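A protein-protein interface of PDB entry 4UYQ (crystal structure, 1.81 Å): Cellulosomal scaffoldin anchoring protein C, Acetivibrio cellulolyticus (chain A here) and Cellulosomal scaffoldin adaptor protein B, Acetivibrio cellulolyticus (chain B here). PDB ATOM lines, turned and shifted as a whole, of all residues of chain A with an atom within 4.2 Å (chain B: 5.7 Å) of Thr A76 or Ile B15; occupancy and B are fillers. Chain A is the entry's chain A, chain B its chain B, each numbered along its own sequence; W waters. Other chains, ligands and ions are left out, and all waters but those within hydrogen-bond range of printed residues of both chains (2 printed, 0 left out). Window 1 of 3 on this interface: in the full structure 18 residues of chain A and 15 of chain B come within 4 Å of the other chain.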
ATOM      1  N   ALA A  33      31.701  23.474  11.200  1.00  0.00           N
ATOM      2  CA  ALA A  33      30.961  22.199  11.049  1.00  0.00           C
ATOM      3  C   ALA A  33      31.085  21.408  12.303  1.00  0.00           C
ATOM      4  O   ALA A  33      32.203  21.335  12.890  1.00  0.00           O
ATOM      5  CB  ALA A  33      31.547  21.384   9.904  1.00  0.00           C
ATOM      6  N   LEU A  34      30.022  20.681  12.599  1.00  0.00           N
ATOM      7  CA  LEU A  34      30.072  19.752  13.706  1.00  0.00           C
ATOM      8  C   LEU A  34      29.101  18.605  13.564  1.00  0.00           C
ATOM      9  O   LEU A  34      28.082  18.754  12.916  1.00  0.00           O
ATOM     10  CB  LEU A  34      29.821  20.490  15.043  1.00  0.00           C
ATOM     11  CG  LEU A  34      28.373  20.950  15.324  1.00  0.00           C
ATOM     12  CD1 LEU A  34      27.674  19.994  16.275  1.00  0.00           C
ATOM     13  CD2 LEU A  34      28.369  22.348  15.929  1.00  0.00           C
ATOM     14  N   SER A  35      29.336  17.517  14.284  1.00  0.00           N
ATOM     15  CA  SER A  35      28.319  16.502  14.496  1.00  0.00           C
ATOM     16  C   SER A  35      28.330  16.172  15.988  1.00  0.00           C
ATOM     17  O   SER A  35      29.397  16.278  16.680  1.00  0.00           O
ATOM     18  CB  SER A  35      28.570  15.203  13.653  1.00  0.00           C
ATOM     19  OG  SER A  35      29.735  14.461  14.076  1.00  0.00           O
ATOM     20  N   ASP A  61      21.053  24.760   7.686  1.00  0.00           N
ATOM     21  CA  ASP A  61      22.397  24.419   8.144  1.00  0.00           C
ATOM     22  C   ASP A  61      22.428  23.199   9.095  1.00  0.00           C
ATOM     23  O   ASP A  61      23.530  22.663   9.348  1.00  0.00           O
ATOM     24  CB  ASP A  61      23.015  25.640   8.871  1.00  0.00           C
ATOM     25  CG  ASP A  61      23.171  26.895   7.979  1.00  0.00           C
ATOM     26  OD1 ASP A  61      23.229  26.757   6.727  1.00  0.00           O
ATOM     27  OD2 ASP A  61      23.302  28.009   8.550  1.00  0.00           O
ATOM     28  N   PHE A  62      21.265  22.806   9.649  1.00  0.00           N
ATOM     29  CA  PHE A  62      21.100  21.916  10.802  1.00  0.00           C
ATOM     30  C   PHE A  62      20.314  20.703  10.331  1.00  0.00           C
ATOM     31  O   PHE A  62      19.225  20.838   9.729  1.00  0.00           O
ATOM     32  CB  PHE A  62      20.241  22.677  11.855  1.00  0.00           C
ATOM     33  CG  PHE A  62      19.971  21.948  13.072  1.00  0.00           C
ATOM     34  CD1 PHE A  62      20.991  21.699  13.951  1.00  0.00           C
ATOM     35  CD2 PHE A  62      18.663  21.550  13.414  1.00  0.00           C
ATOM     36  CE1 PHE A  62      20.722  21.079  15.152  1.00  0.00           C
ATOM     37  CE2 PHE A  62      18.385  20.961  14.601  1.00  0.00           C
ATOM     38  CZ  PHE A  62      19.428  20.675  15.466  1.00  0.00           C
ATOM     39  N   THR A  63      20.817  19.507  10.608  1.00  0.00           N
ATOM     40  CA  THR A  63      20.133  18.258  10.291  1.00  0.00           C
ATOM     41  C   THR A  63      20.143  17.335  11.512  1.00  0.00           C
ATOM     42  O   THR A  63      21.118  17.288  12.220  1.00  0.00           O
ATOM     43  CB  THR A  63      20.848  17.556   9.118  1.00  0.00           C
ATOM     44  OG1 THR A  63      21.147  18.526   8.115  1.00  0.00           O
ATOM     45  CG2 THR A  63      19.920  16.501   8.432  1.00  0.00           C
ATOM     46  N   MET A  75      22.948  14.990  15.457  1.00  0.00           N
ATOM     47  CA  MET A  75      22.726  16.354  14.999  1.00  0.00           C
ATOM     48  C   MET A  75      23.966  16.784  14.241  1.00  0.00           C
ATOM     49  O   MET A  75      25.089  16.493  14.697  1.00  0.00           O
ATOM     50  CB  MET A  75      22.553  17.319  16.157  1.00  0.00           C
ATOM     51  CG  MET A  75      21.241  17.144  16.933  1.00  0.00           C
ATOM     52  SD  MET A  75      21.374  17.029  18.752  1.00  0.00           S
ATOM     53  CE  MET A  75      21.827  15.298  18.986  1.00  0.00           C
ATOM     54  N   THR A  76      23.767  17.479  13.101  1.00  0.00           N
ATOM     55  CA  THR A  76      24.850  18.079  12.350  1.00  0.00           C
ATOM     56  C   THR A  76      24.596  19.561  12.110  1.00  0.00           C
ATOM     57  O   THR A  76      23.471  19.992  11.986  1.00  0.00           O
ATOM     58  CB  THR A  76      25.219  17.426  11.002  1.00  0.00           C
ATOM     59  OG1 THR A  76      24.105  17.498  10.065  1.00  0.00           O
ATOM     60  CG2 THR A  76      25.696  15.983  11.170  1.00  0.00           C
ATOM     61  N   PHE A  77      25.674  20.312  12.085  1.00  0.00           N
ATOM     62  CA  PHE A  77      25.699  21.685  11.595  1.00  0.00           C
ATOM     63  C   PHE A  77      26.766  21.852  10.562  1.00  0.00           C
ATOM     64  O   PHE A  77      27.952  21.437  10.766  1.00  0.00           O
ATOM     65  CB  PHE A  77      25.939  22.684  12.746  1.00  0.00           C
ATOM     66  CG  PHE A  77      26.157  24.082  12.312  1.00  0.00           C
ATOM     67  CD1 PHE A  77      25.083  24.868  11.971  1.00  0.00           C
ATOM     68  CD2 PHE A  77      27.409  24.634  12.341  1.00  0.00           C
ATOM     69  CE1 PHE A  77      25.269  26.179  11.575  1.00  0.00           C
ATOM     70  CE2 PHE A  77      27.624  25.950  11.937  1.00  0.00           C
ATOM     71  CZ  PHE A  77      26.547  26.708  11.557  1.00  0.00           C
ATOM     72  N   GLU A  78      26.415  22.506   9.457  1.00  0.00           N
ATOM     73  CA  GLU A  78      27.354  22.815   8.399  1.00  0.00           C
ATOM     74  C   GLU A  78      27.146  24.300   8.019  1.00  0.00           C
ATOM     75  O   GLU A  78      26.086  24.682   7.498  1.00  0.00           O
ATOM     76  CB  GLU A  78      27.079  21.941   7.171  1.00  0.00           C
ATOM     77  CG  GLU A  78      26.996  20.411   7.441  1.00  0.00           C
ATOM     78  CD  GLU A  78      26.182  19.667   6.409  1.00  0.00           C
ATOM     79  OE1 GLU A  78      24.911  19.887   6.321  1.00  0.00           O
ATOM     80  OE2 GLU A  78      26.834  18.827   5.692  1.00  0.00           O
ATOM     81  N   SER A 120      32.253  15.431  16.438  1.00  0.00           N
ATOM     82  CA  SER A 120      33.473  16.195  16.193  1.00  0.00           C
ATOM     83  C   SER A 120      33.089  17.598  15.824  1.00  0.00           C
ATOM     84  O   SER A 120      31.935  17.878  15.460  1.00  0.00           O
ATOM     85  CB  SER A 120      34.321  15.537  15.057  1.00  0.00           C
ATOM     86  OG  SER A 120      33.641  15.612  13.841  1.00  0.00           O
ATOM     87  N   VAL B  13      35.208   8.584   8.882  1.00  0.00           N
ATOM     88  CA  VAL B  13      34.237   9.370   8.169  1.00  0.00           C
ATOM     89  C   VAL B  13      33.584  10.328   9.203  1.00  0.00           C
ATOM     90  O   VAL B  13      33.033   9.908  10.226  1.00  0.00           O
ATOM     91  CB  VAL B  13      33.137   8.534   7.518  1.00  0.00           C
ATOM     92  CG1 VAL B  13      32.156   9.427   6.802  1.00  0.00           C
ATOM     93  CG2 VAL B  13      33.753   7.560   6.531  1.00  0.00           C
ATOM     94  N   ARG B  14      33.775  11.616   8.980  1.00  0.00           N
ATOM     95  CA  ARG B  14      33.278  12.669   9.860  1.00  0.00           C
ATOM     96  C   ARG B  14      32.611  13.786   9.085  1.00  0.00           C
ATOM     97  O   ARG B  14      32.642  13.867   7.823  1.00  0.00           O
ATOM     98  CB  ARG B  14      34.464  13.295  10.670  1.00  0.00           C
ATOM     99  CG  ARG B  14      35.297  12.366  11.486  1.00  0.00           C
ATOM    100  CD  ARG B  14      36.387  13.143  12.217  1.00  0.00           C
ATOM    101  NE  ARG B  14      37.184  12.316  13.115  1.00  0.00           N
ATOM    102  CZ  ARG B  14      38.214  12.740  13.821  1.00  0.00           C
ATOM    103  NH1 ARG B  14      38.712  13.923  13.600  1.00  0.00           N
ATOM    104  NH2 ARG B  14      38.826  11.911  14.648  1.00  0.00           N
ATOM    105  N   ILE B  15      31.987  14.703   9.842  1.00  0.00           N
ATOM    106  CA  ILE B  15      31.276  15.808   9.230  1.00  0.00           C
ATOM    107  C   ILE B  15      32.164  16.625   8.335  1.00  0.00           C
ATOM    108  O   ILE B  15      31.704  17.130   7.349  1.00  0.00           O
ATOM    109  CB  ILE B  15      30.562  16.697  10.344  1.00  0.00           C
ATOM    110  CG1 ILE B  15      29.534  17.627   9.695  1.00  0.00           C
ATOM    111  CG2 ILE B  15      31.570  17.469  11.158  1.00  0.00           C
ATOM    112  CD1 ILE B  15      28.502  16.884   8.881  1.00  0.00           C
ATOM    113  N   ASN B  16      33.474  16.785   8.668  1.00  0.00           N
ATOM    114  CA  ASN B  16      34.313  17.666   7.811  1.00  0.00           C
ATOM    115  C   ASN B  16      34.550  17.040   6.434  1.00  0.00           C
ATOM    116  O   ASN B  16      34.760  17.728   5.460  1.00  0.00           O
ATOM    117  CB  ASN B  16      35.652  17.997   8.455  1.00  0.00           C
ATOM    118  CG  ASN B  16      36.604  16.805   8.487  1.00  0.00           C
ATOM    119  OD1 ASN B  16      36.271  15.770   9.046  1.00  0.00           O
ATOM    120  ND2 ASN B  16      37.781  16.980   7.976  1.00  0.00           N
ATOM    121  N   ASP B  17      34.443  15.704   6.348  1.00  0.00           N
ATOM    122  CA  ASP B  17      34.579  15.011   5.068  1.00  0.00           C
ATOM    123  C   ASP B  17      33.374  15.432   4.194  1.00  0.00           C
ATOM    124  O   ASP B  17      33.560  15.694   3.014  1.00  0.00           O
ATOM    125  CB  ASP B  17      34.604  13.454   5.271  1.00  0.00           C
ATOM    126  CG  ASP B  17      35.848  12.995   6.023  1.00  0.00           C
ATOM    127  OD1 ASP B  17      37.013  13.190   5.554  1.00  0.00           O
ATOM    128  OD2 ASP B  17      35.698  12.338   7.060  1.00  0.00           O
ATOM    129  N   ALA B  18      32.169  15.526   4.771  1.00  0.00           N
ATOM    130  CA  ALA B  18      31.001  15.942   4.012  1.00  0.00           C
ATOM    131  C   ALA B  18      31.187  17.363   3.502  1.00  0.00           C
ATOM    132  O   ALA B  18      30.961  17.647   2.333  1.00  0.00           O
ATOM    133  CB  ALA B  18      29.722  15.821   4.854  1.00  0.00           C
ATOM    134  N   VAL B  19      31.663  18.241   4.385  1.00  0.00           N
ATOM    135  CA  VAL B  19      31.849  19.632   4.026  1.00  0.00           C
ATOM    136  C   VAL B  19      32.988  19.861   3.009  1.00  0.00           C
ATOM    137  O   VAL B  19      32.877  20.766   2.084  1.00  0.00           O
ATOM    138  CB  VAL B  19      31.941  20.486   5.317  1.00  0.00           C
ATOM    139  CG1 VAL B  19      32.350  21.907   5.007  1.00  0.00           C
ATOM    140  CG2 VAL B  19      30.612  20.408   6.065  1.00  0.00           C
ATOM    141  N   LEU B  20      34.058  19.091   3.115  1.00  0.00           N
ATOM    142  CA  LEU B  20      35.080  19.077   2.045  1.00  0.00           C
ATOM    143  C   LEU B  20      34.511  18.700   0.672  1.00  0.00           C
ATOM    144  O   LEU B  20      34.824  19.383  -0.323  1.00  0.00           O
ATOM    145  CB  LEU B  20      36.264  18.195   2.400  1.00  0.00           C
ATOM    146  CG  LEU B  20      37.226  18.716   3.507  1.00  0.00           C
ATOM    147  CD1 LEU B  20      38.150  17.600   3.942  1.00  0.00           C
ATOM    148  CD2 LEU B  20      38.012  19.970   3.046  1.00  0.00           C
ATOM    149  N   ARG B  58      27.135  13.079   4.986  1.00  0.00           N
ATOM    150  CA  ARG B  58      26.346  13.532   6.145  1.00  0.00           C
ATOM    151  C   ARG B  58      25.410  12.449   6.694  1.00  0.00           C
ATOM    152  O   ARG B  58      25.341  12.226   7.917  1.00  0.00           O
ATOM    153  CB  ARG B  58      25.631  14.839   5.895  1.00  0.00           C
ATOM    154  CG  ARG B  58      24.907  15.365   7.143  1.00  0.00           C
ATOM    155  CD  ARG B  58      24.230  16.656   6.708  1.00  0.00           C
ATOM    156  NE  ARG B  58      23.122  16.393   5.871  1.00  0.00           N
ATOM    157  CZ  ARG B  58      22.605  17.244   4.964  1.00  0.00           C
ATOM    158  NH1 ARG B  58      23.035  18.474   4.766  1.00  0.00           N
ATOM    159  NH2 ARG B  58      21.585  16.844   4.265  1.00  0.00           N
ATOM    160  N   VAL B  61      27.316  10.003   8.819  1.00  0.00           N
ATOM    161  CA  VAL B  61      27.591  10.614  10.111  1.00  0.00           C
ATOM    162  C   VAL B  61      26.359  10.663  11.034  1.00  0.00           C
ATOM    163  O   VAL B  61      26.543  10.397  12.210  1.00  0.00           O
ATOM    164  CB  VAL B  61      28.257  11.980   9.899  1.00  0.00           C
ATOM    165  CG1 VAL B  61      28.482  12.647  11.268  1.00  0.00           C
ATOM    166  CG2 VAL B  61      29.566  11.837   9.138  1.00  0.00           C
ATOM    167  N   LEU B  62      25.162  10.948  10.509  1.00  0.00           N
ATOM    168  CA  LEU B  62      23.919  10.958  11.217  1.00  0.00           C
ATOM    169  C   LEU B  62      23.514   9.579  11.669  1.00  0.00           C
ATOM    170  O   LEU B  62      22.715   9.431  12.616  1.00  0.00           O
ATOM    171  CB  LEU B  62      22.812  11.583  10.416  1.00  0.00           C
ATOM    172  CG  LEU B  62      22.909  13.098  10.147  1.00  0.00           C
ATOM    173  CD1 LEU B  62      21.998  13.551   9.039  1.00  0.00           C
ATOM    174  CD2 LEU B  62      22.490  13.790  11.422  1.00  0.00           C
HETATM  175  O   HOH W   1      31.850  13.945  12.736  1.00  0.00           O
HETATM  176  O   HOH W   2      28.165  19.373   3.467  1.00  0.00           O
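Leu A34 touches Ile B15. Ser A35 touches Ile B15 (N to CG2, 3.8 Å). CB of Ser A35 touches CG1 of Val B61, 3.5 Å away. Arg B58 touches Thr A63 (NE to OG1, 3.7 Å). Thr A63 touches Leu B62 (CG2 to CD1, 3.7 Å). Thr A76 touches Ile B15. OG1 of Thr A76 touches CD of Arg B58, 3.5 Å away. CD2 of Leu B62 touches CG2 of Thr A76, at 3.9 Å. Glu A78 touches Val B19. Ile B15 touches Ser A120 (CG2 to OG, 3.9 Å).
Printed residues of chain B within 4 Å of Leu A34: Ile B15 (3.6 Å). Of the printed residues of chain B, Glu A78 touches Val B19 and Arg B58. Of chain A, only Leu A34 (3.6 Å), Ser A35 (3.8 Å), Thr A76 (3.7 Å) and Ser A120 (3.9 Å) come within 4 Å of Ile B15. Ala B18 touches none of the printed residues of chain A. Printed residues of chain A within 4 Å of Val B19: Glu A78. Printed residues of chain A within 4 Å of Arg B58: Thr A63 (3.7 Å), Thr A76 (3.5 Å) and Glu A78 (2.8 Å). Printed residues of chain A within 4 Å of Val B61: Ser A35 (3.5 Å). The nearest residue of chain B that does not touch Thr A76 is Val B61 (4.3 Å). The nearest printed residue of chain A that does not touch Ile B15 is Glu A78 (4.1 Å). The nearest printed residue of chain A that does not touch Arg B58 is Asp A61 (6.2 Å).
N of Leu A34 lies within hydrogen-bond range of O of Phe A77. The backbone carbonyl oxygen (O) of Ser A120 sits at hydrogen-bond distance from the backbone NH (N) of Ser A35. The backbone carbonyl oxygen (O) of Asp A61 sits at hydrogen-bond distance from the backbone NH (N) of Glu A78, at 2.9 Å. O of Thr A63 lies within hydrogen-bond range of N of Thr A76 (2.8 Å).
NH1 of Arg B58 is in salt-bridge range of OE1 of Glu A78 (2.8 Å).
Water W1 lies within hydrogen-bond range of the side-chain hydroxyl (OG) of Ser A35, the side-chain hydroxyl (OG) of Ser A120 and the backbone NH (N) of Ile B15. Water W2 lies within hydrogen-bond range of OE2 of Glu A78 and O of Ala B18.
Among the printed residues, Asp or Glu carboxylates within 4 Å of a Lys or Arg side-chain nitrogen of the other chain: Glu A78 with Arg B58 (2.8 Å).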
